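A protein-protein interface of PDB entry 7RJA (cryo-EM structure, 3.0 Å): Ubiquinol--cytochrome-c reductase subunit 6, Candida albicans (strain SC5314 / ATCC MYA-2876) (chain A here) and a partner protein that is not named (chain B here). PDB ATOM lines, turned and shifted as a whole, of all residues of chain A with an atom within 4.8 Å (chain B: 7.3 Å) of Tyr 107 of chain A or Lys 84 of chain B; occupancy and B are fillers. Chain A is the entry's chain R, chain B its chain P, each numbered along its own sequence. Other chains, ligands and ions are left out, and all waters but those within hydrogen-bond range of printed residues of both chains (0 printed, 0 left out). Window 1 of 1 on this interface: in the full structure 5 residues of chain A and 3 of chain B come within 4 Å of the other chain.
The side-chain carboxylate (OE1) of Glu 113 of chain A is in hydrogen-bond range of the backbone NH (N) of Lys 84 of chain B.
The side-chain amino group (NZ) of Lys 84 of chain B is in salt-bridge range of the side-chain carboxylate (OE1) of Glu 114 of chain A.
Of the 9 printed residues of chain A, 5 touch a printed residue of chain B.
Printed residues of chain A that touch a printed residue of chain B: Tyr 107, Glu 109, Asp 110, Glu 113 and Glu 114.
Hydrophobic or aromatic side chains of chain A within 4 Å of the printed part of chain B: Tyr 107.
Of the 10 printed residues of chain B, 3 touch a printed residue of chain A.
Among the printed residues, 7 pairs touch across the chains.
Among the printed residues, pairs that only touch across the chains: Glu 113 of chain A with Thr 83 of chain B, Tyr 107 of chain A with Arg 87 of chain B, Tyr 107 of chain A with Lys 84 of chain B, Asp 110 of chain A with Lys 84 of chain B and Glu 109 of chain A with Lys 84 of chain B.
Tyr 107 of chain A touches two residues of chain B.
Printed residues of chain B within 4 Å of Glu 113 of chain A: Thr 83 (3.1 Å) and Lys 84 (3.2 Å).
Of the printed residues of chain B, Asp 110 of chain A touches Lys 84.
Of the printed residues of chain A, Arg 87 of chain B touches Tyr 107.
Of the printed residues of chain A, Thr 83 of chain B touches Glu 113 (3.1 Å).
Printed residues of chain B within 4 Å of Glu 114 of chain A: Lys 84 (2.5 Å).
The nearest residue of chain A that does not touch Lys 84 of chain B is Arg 92 of chain A (4.6 Å).
The backbone carbonyl oxygen (O) of Tyr 80 of chain B is in hydrogen-bond range of the side-chain hydroxyl (OG1) of Thr 83 of chain B, 2.6 Å away.
The side-chain carboxylate of Glu 85 of chain B sits at hydrogen-bond distance from the side-chain hydroxyl of Thr 83 of chain B (2.5 Å).
The side-chain hydroxyl (OG1) of Thr 83 of chain B lies within hydrogen-bond range of the backbone NH (N) of Gly 86 of chain B (3.3 Å).
The guanidinium group of Arg 92 of chain A lies within salt-bridge range of the side-chain carboxylate of Glu 109 of chain A, at 2.5 Å.
The side-chain carboxylate (OE2) of Glu 114 of chain A is in salt-bridge range of the guanidinium group (NH2) of Arg 92 of chain A (3.7 Å).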
ATOM      1  N   ARG A  92      -6.516 -32.524 -34.238  1.00  0.00           N
ATOM      2  CA  ARG A  92      -5.206 -33.164 -34.285  1.00  0.00           C
ATOM      3  C   ARG A  92      -4.865 -33.822 -32.954  1.00  0.00           C
ATOM      4  O   ARG A  92      -4.308 -34.926 -32.922  1.00  0.00           O
ATOM      5  CB  ARG A  92      -4.132 -32.147 -34.663  1.00  0.00           C
ATOM      6  CG  ARG A  92      -2.751 -32.760 -34.842  1.00  0.00           C
ATOM      7  CD  ARG A  92      -1.762 -31.769 -35.427  1.00  0.00           C
ATOM      8  NE  ARG A  92      -1.515 -30.649 -34.527  1.00  0.00           N
ATOM      9  CZ  ARG A  92      -2.210 -29.519 -34.523  1.00  0.00           C
ATOM     10  NH1 ARG A  92      -3.199 -29.308 -35.376  1.00  0.00           N
ATOM     11  NH2 ARG A  92      -1.903 -28.573 -33.640  1.00  0.00           N
ATOM     12  N   LYS A 105       4.216 -41.357 -25.371  1.00  0.00           N
ATOM     13  CA  LYS A 105       4.821 -40.208 -26.033  1.00  0.00           C
ATOM     14  C   LYS A 105       5.377 -39.225 -25.012  1.00  0.00           C
ATOM     15  O   LYS A 105       4.714 -38.888 -24.027  1.00  0.00           O
ATOM     16  CB  LYS A 105       3.792 -39.515 -26.923  1.00  0.00           C
ATOM     17  CG  LYS A 105       3.361 -40.335 -28.122  1.00  0.00           C
ATOM     18  CD  LYS A 105       2.362 -39.578 -28.979  1.00  0.00           C
ATOM     19  CE  LYS A 105       1.914 -40.407 -30.169  1.00  0.00           C
ATOM     20  NZ  LYS A 105       0.924 -39.685 -31.014  1.00  0.00           N
ATOM     21  N   HIS A 106       6.607 -38.769 -25.252  1.00  0.00           N
ATOM     22  CA  HIS A 106       7.208 -37.767 -24.379  1.00  0.00           C
ATOM     23  C   HIS A 106       6.513 -36.422 -24.537  1.00  0.00           C
ATOM     24  O   HIS A 106       6.184 -35.760 -23.546  1.00  0.00           O
ATOM     25  CB  HIS A 106       8.700 -37.639 -24.681  1.00  0.00           C
ATOM     26  CG  HIS A 106       9.557 -38.583 -23.899  1.00  0.00           C
ATOM     27  ND1 HIS A 106      10.141 -38.238 -22.699  1.00  0.00           N
ATOM     28  CD2 HIS A 106       9.928 -39.862 -24.144  1.00  0.00           C
ATOM     29  CE1 HIS A 106      10.835 -39.264 -22.239  1.00  0.00           C
ATOM     30  NE2 HIS A 106      10.723 -40.261 -23.097  1.00  0.00           N
ATOM     31  N   TYR A 107       6.282 -36.003 -25.778  1.00  0.00           N
ATOM     32  CA  TYR A 107       5.618 -34.737 -26.076  1.00  0.00           C
ATOM     33  C   TYR A 107       4.184 -35.037 -26.496  1.00  0.00           C
ATOM     34  O   TYR A 107       3.924 -35.391 -27.649  1.00  0.00           O
ATOM     35  CB  TYR A 107       6.363 -33.975 -27.164  1.00  0.00           C
ATOM     36  CG  TYR A 107       5.659 -32.712 -27.600  1.00  0.00           C
ATOM     37  CD1 TYR A 107       5.415 -32.459 -28.940  1.00  0.00           C
ATOM     38  CD2 TYR A 107       5.235 -31.777 -26.668  1.00  0.00           C
ATOM     39  CE1 TYR A 107       4.770 -31.308 -29.342  1.00  0.00           C
ATOM     40  CE2 TYR A 107       4.589 -30.623 -27.059  1.00  0.00           C
ATOM     41  CZ  TYR A 107       4.359 -30.393 -28.397  1.00  0.00           C
ATOM     42  OH  TYR A 107       3.716 -29.244 -28.792  1.00  0.00           O
ATOM     43  N   LYS A 108       3.255 -34.889 -25.559  1.00  0.00           N
ATOM     44  CA  LYS A 108       1.832 -35.076 -25.821  1.00  0.00           C
ATOM     45  C   LYS A 108       1.245 -33.700 -26.109  1.00  0.00           C
ATOM     46  O   LYS A 108       1.060 -32.888 -25.199  1.00  0.00           O
ATOM     47  CB  LYS A 108       1.154 -35.753 -24.636  1.00  0.00           C
ATOM     48  CG  LYS A 108       1.277 -37.267 -24.659  1.00  0.00           C
ATOM     49  CD  LYS A 108       0.619 -37.907 -23.451  1.00  0.00           C
ATOM     50  CE  LYS A 108       1.605 -38.079 -22.310  1.00  0.00           C
ATOM     51  NZ  LYS A 108       2.652 -39.091 -22.625  1.00  0.00           N
ATOM     52  N   GLU A 109       0.956 -33.440 -27.381  1.00  0.00           N
ATOM     53  CA  GLU A 109       0.575 -32.102 -27.802  1.00  0.00           C
ATOM     54  C   GLU A 109      -0.710 -31.662 -27.112  1.00  0.00           C
ATOM     55  O   GLU A 109      -1.550 -32.473 -26.717  1.00  0.00           O
ATOM     56  CB  GLU A 109       0.393 -32.049 -29.317  1.00  0.00           C
ATOM     57  CG  GLU A 109       0.198 -30.645 -29.863  1.00  0.00           C
ATOM     58  CD  GLU A 109       0.240 -30.596 -31.377  1.00  0.00           C
ATOM     59  OE1 GLU A 109       1.006 -31.377 -31.976  1.00  0.00           O
ATOM     60  OE2 GLU A 109      -0.497 -29.779 -31.967  1.00  0.00           O
ATOM     61  N   ASP A 110      -0.849 -30.348 -26.967  1.00  0.00           N
ATOM     62  CA  ASP A 110      -2.029 -29.755 -26.361  1.00  0.00           C
ATOM     63  C   ASP A 110      -2.319 -28.432 -27.051  1.00  0.00           C
ATOM     64  O   ASP A 110      -1.420 -27.778 -27.586  1.00  0.00           O
ATOM     65  CB  ASP A 110      -1.842 -29.564 -24.852  1.00  0.00           C
ATOM     66  CG  ASP A 110      -0.716 -28.606 -24.522  1.00  0.00           C
ATOM     67  OD1 ASP A 110      -0.048 -28.117 -25.456  1.00  0.00           O
ATOM     68  OD2 ASP A 110      -0.489 -28.350 -23.322  1.00  0.00           O
ATOM     69  N   GLU A 113      -2.035 -23.212 -26.566  1.00  0.00           N
ATOM     70  CA  GLU A 113      -1.587 -22.002 -27.248  1.00  0.00           C
ATOM     71  C   GLU A 113      -2.663 -21.459 -28.181  1.00  0.00           C
ATOM     72  O   GLU A 113      -2.929 -20.251 -28.203  1.00  0.00           O
ATOM     73  CB  GLU A 113      -0.301 -22.280 -28.022  1.00  0.00           C
ATOM     74  CG  GLU A 113       0.534 -21.039 -28.276  1.00  0.00           C
ATOM     75  CD  GLU A 113       1.616 -21.269 -29.309  1.00  0.00           C
ATOM     76  OE1 GLU A 113       2.671 -21.830 -28.949  1.00  0.00           O
ATOM     77  OE2 GLU A 113       1.414 -20.888 -30.481  1.00  0.00           O
ATOM     78  N   GLU A 114      -3.285 -22.333 -28.974  1.00  0.00           N
ATOM     79  CA  GLU A 114      -4.366 -21.880 -29.843  1.00  0.00           C
ATOM     80  C   GLU A 114      -5.533 -21.353 -29.022  1.00  0.00           C
ATOM     81  O   GLU A 114      -6.152 -20.342 -29.379  1.00  0.00           O
ATOM     82  CB  GLU A 114      -4.826 -23.018 -30.751  1.00  0.00           C
ATOM     83  CG  GLU A 114      -3.828 -23.386 -31.825  1.00  0.00           C
ATOM     84  CD  GLU A 114      -2.799 -24.375 -31.334  1.00  0.00           C
ATOM     85  OE1 GLU A 114      -2.510 -24.370 -30.120  1.00  0.00           O
ATOM     86  OE2 GLU A 114      -2.275 -25.154 -32.158  1.00  0.00           O
ATOM     87  N   GLU B  79       9.974 -15.289 -27.192  1.00  0.00           N
ATOM     88  CA  GLU B  79       8.591 -15.666 -27.451  1.00  0.00           C
ATOM     89  C   GLU B  79       8.526 -16.884 -28.358  1.00  0.00           C
ATOM     90  O   GLU B  79       7.706 -17.783 -28.147  1.00  0.00           O
ATOM     91  CB  GLU B  79       7.831 -14.499 -28.078  1.00  0.00           C
ATOM     92  CG  GLU B  79       7.601 -13.329 -27.142  1.00  0.00           C
ATOM     93  CD  GLU B  79       6.387 -12.507 -27.526  1.00  0.00           C
ATOM     94  OE1 GLU B  79       5.955 -12.593 -28.694  1.00  0.00           O
ATOM     95  OE2 GLU B  79       5.865 -11.774 -26.660  1.00  0.00           O
ATOM     96  N   TYR B  80       9.387 -16.931 -29.372  1.00  0.00           N
ATOM     97  CA  TYR B  80       9.370 -18.051 -30.303  1.00  0.00           C
ATOM     98  C   TYR B  80       9.748 -19.351 -29.607  1.00  0.00           C
ATOM     99  O   TYR B  80       9.187 -20.408 -29.910  1.00  0.00           O
ATOM    100  CB  TYR B  80      10.315 -17.772 -31.466  1.00  0.00           C
ATOM    101  CG  TYR B  80      10.807 -19.010 -32.169  1.00  0.00           C
ATOM    102  CD1 TYR B  80      10.038 -19.630 -33.138  1.00  0.00           C
ATOM    103  CD2 TYR B  80      12.038 -19.561 -31.862  1.00  0.00           C
ATOM    104  CE1 TYR B  80      10.484 -20.759 -33.787  1.00  0.00           C
ATOM    105  CE2 TYR B  80      12.492 -20.690 -32.501  1.00  0.00           C
ATOM    106  CZ  TYR B  80      11.712 -21.287 -33.463  1.00  0.00           C
ATOM    107  OH  TYR B  80      12.162 -22.416 -34.106  1.00  0.00           O
ATOM    108  N   LEU B  81      10.701 -19.296 -28.674  1.00  0.00           N
ATOM    109  CA  LEU B  81      11.157 -20.521 -28.026  1.00  0.00           C
ATOM    110  C   LEU B  81      10.032 -21.204 -27.261  1.00  0.00           C
ATOM    111  O   LEU B  81       9.889 -22.431 -27.322  1.00  0.00           O
ATOM    112  CB  LEU B  81      12.322 -20.219 -27.085  1.00  0.00           C
ATOM    113  CG  LEU B  81      13.681 -19.921 -27.713  1.00  0.00           C
ATOM    114  CD1 LEU B  81      14.735 -19.960 -26.639  1.00  0.00           C
ATOM    115  CD2 LEU B  81      14.023 -20.899 -28.820  1.00  0.00           C
ATOM    116  N   TYR B  82       9.229 -20.436 -26.530  1.00  0.00           N
ATOM    117  CA  TYR B  82       8.191 -21.010 -25.673  1.00  0.00           C
ATOM    118  C   TYR B  82       6.885 -21.133 -26.460  1.00  0.00           C
ATOM    119  O   TYR B  82       5.863 -20.515 -26.159  1.00  0.00           O
ATOM    120  CB  TYR B  82       8.022 -20.177 -24.410  1.00  0.00           C
ATOM    121  CG  TYR B  82       9.221 -20.239 -23.492  1.00  0.00           C
ATOM    122  CD1 TYR B  82       9.102 -20.723 -22.199  1.00  0.00           C
ATOM    123  CD2 TYR B  82      10.471 -19.819 -23.916  1.00  0.00           C
ATOM    124  CE1 TYR B  82      10.190 -20.786 -21.359  1.00  0.00           C
ATOM    125  CE2 TYR B  82      11.564 -19.877 -23.082  1.00  0.00           C
ATOM    126  CZ  TYR B  82      11.418 -20.362 -21.805  1.00  0.00           C
ATOM    127  OH  TYR B  82      12.506 -20.422 -20.969  1.00  0.00           O
ATOM    128  N   THR B  83       6.946 -21.970 -27.493  1.00  0.00           N
ATOM    129  CA  THR B  83       5.792 -22.286 -28.320  1.00  0.00           C
ATOM    130  C   THR B  83       5.958 -23.705 -28.842  1.00  0.00           C
ATOM    131  O   THR B  83       7.053 -24.272 -28.808  1.00  0.00           O
ATOM    132  CB  THR B  83       5.640 -21.306 -29.488  1.00  0.00           C
ATOM    133  OG1 THR B  83       6.811 -21.359 -30.310  1.00  0.00           O
ATOM    134  CG2 THR B  83       5.441 -19.891 -28.983  1.00  0.00           C
ATOM    135  N   LYS B  84       4.858 -24.276 -29.333  1.00  0.00           N
ATOM    136  CA  LYS B  84       4.901 -25.661 -29.789  1.00  0.00           C
ATOM    137  C   LYS B  84       5.953 -25.879 -30.867  1.00  0.00           C
ATOM    138  O   LYS B  84       6.568 -26.950 -30.904  1.00  0.00           O
ATOM    139  CB  LYS B  84       3.533 -26.095 -30.313  1.00  0.00           C
ATOM    140  CG  LYS B  84       2.463 -26.192 -29.244  1.00  0.00           C
ATOM    141  CD  LYS B  84       1.195 -26.845 -29.776  1.00  0.00           C
ATOM    142  CE  LYS B  84       0.472 -25.957 -30.767  1.00  0.00           C
ATOM    143  NZ  LYS B  84      -0.034 -24.722 -30.126  1.00  0.00           N
ATOM    144  N   GLU B  85       6.182 -24.897 -31.738  1.00  0.00           N
ATOM    145  CA  GLU B  85       7.205 -25.035 -32.766  1.00  0.00           C
ATOM    146  C   GLU B  85       8.592 -24.659 -32.270  1.00  0.00           C
ATOM    147  O   GLU B  85       9.582 -25.000 -32.925  1.00  0.00           O
ATOM    148  CB  GLU B  85       6.855 -24.184 -33.995  1.00  0.00           C
ATOM    149  CG  GLU B  85       7.030 -22.679 -33.830  1.00  0.00           C
ATOM    150  CD  GLU B  85       6.002 -22.068 -32.909  1.00  0.00           C
ATOM    151  OE1 GLU B  85       5.098 -22.804 -32.460  1.00  0.00           O
ATOM    152  OE2 GLU B  85       6.094 -20.854 -32.632  1.00  0.00           O
ATOM    153  N   GLY B  86       8.688 -23.968 -31.140  1.00  0.00           N
ATOM    154  CA  GLY B  86       9.960 -23.676 -30.522  1.00  0.00           C
ATOM    155  C   GLY B  86      10.411 -24.690 -29.501  1.00  0.00           C
ATOM    156  O   GLY B  86      11.464 -24.507 -28.884  1.00  0.00           O
ATOM    157  N   ARG B  87       9.644 -25.761 -29.298  1.00  0.00           N
ATOM    158  CA  ARG B  87       9.986 -26.728 -28.259  1.00  0.00           C
ATOM    159  C   ARG B  87      11.341 -27.369 -28.528  1.00  0.00           C
ATOM    160  O   ARG B  87      12.183 -27.469 -27.629  1.00  0.00           O
ATOM    161  CB  ARG B  87       8.899 -27.797 -28.165  1.00  0.00           C
ATOM    162  CG  ARG B  87       9.135 -28.817 -27.064  1.00  0.00           C
ATOM    163  CD  ARG B  87       8.024 -29.847 -27.014  1.00  0.00           C
ATOM    164  NE  ARG B  87       7.965 -30.626 -28.245  1.00  0.00           N
ATOM    165  CZ  ARG B  87       8.728 -31.680 -28.504  1.00  0.00           C
ATOM    166  NH1 ARG B  87       9.625 -32.117 -27.635  1.00  0.00           N
ATOM    167  NH2 ARG B  87       8.590 -32.308 -29.668  1.00  0.00           N
ATOM    168  N   GLU B  88      11.571 -27.816 -29.764  1.00  0.00           N
ATOM    169  CA  GLU B  88      12.821 -28.498 -30.073  1.00  0.00           C
ATOM    170  C   GLU B  88      14.015 -27.567 -29.893  1.00  0.00           C
ATOM    171  O   GLU B  88      15.043 -27.963 -29.328  1.00  0.00           O
ATOM    172  CB  GLU B  88      12.772 -29.064 -31.495  1.00  0.00           C
ATOM    173  CG  GLU B  88      13.028 -28.061 -32.617  1.00  0.00           C
ATOM    174  CD  GLU B  88      11.934 -27.022 -32.736  1.00  0.00           C
ATOM    175  OE1 GLU B  88      11.950 -26.251 -33.718  1.00  0.00           O
ATOM    176  OE2 GLU B  88      11.060 -26.972 -31.845  1.00  0.00           O
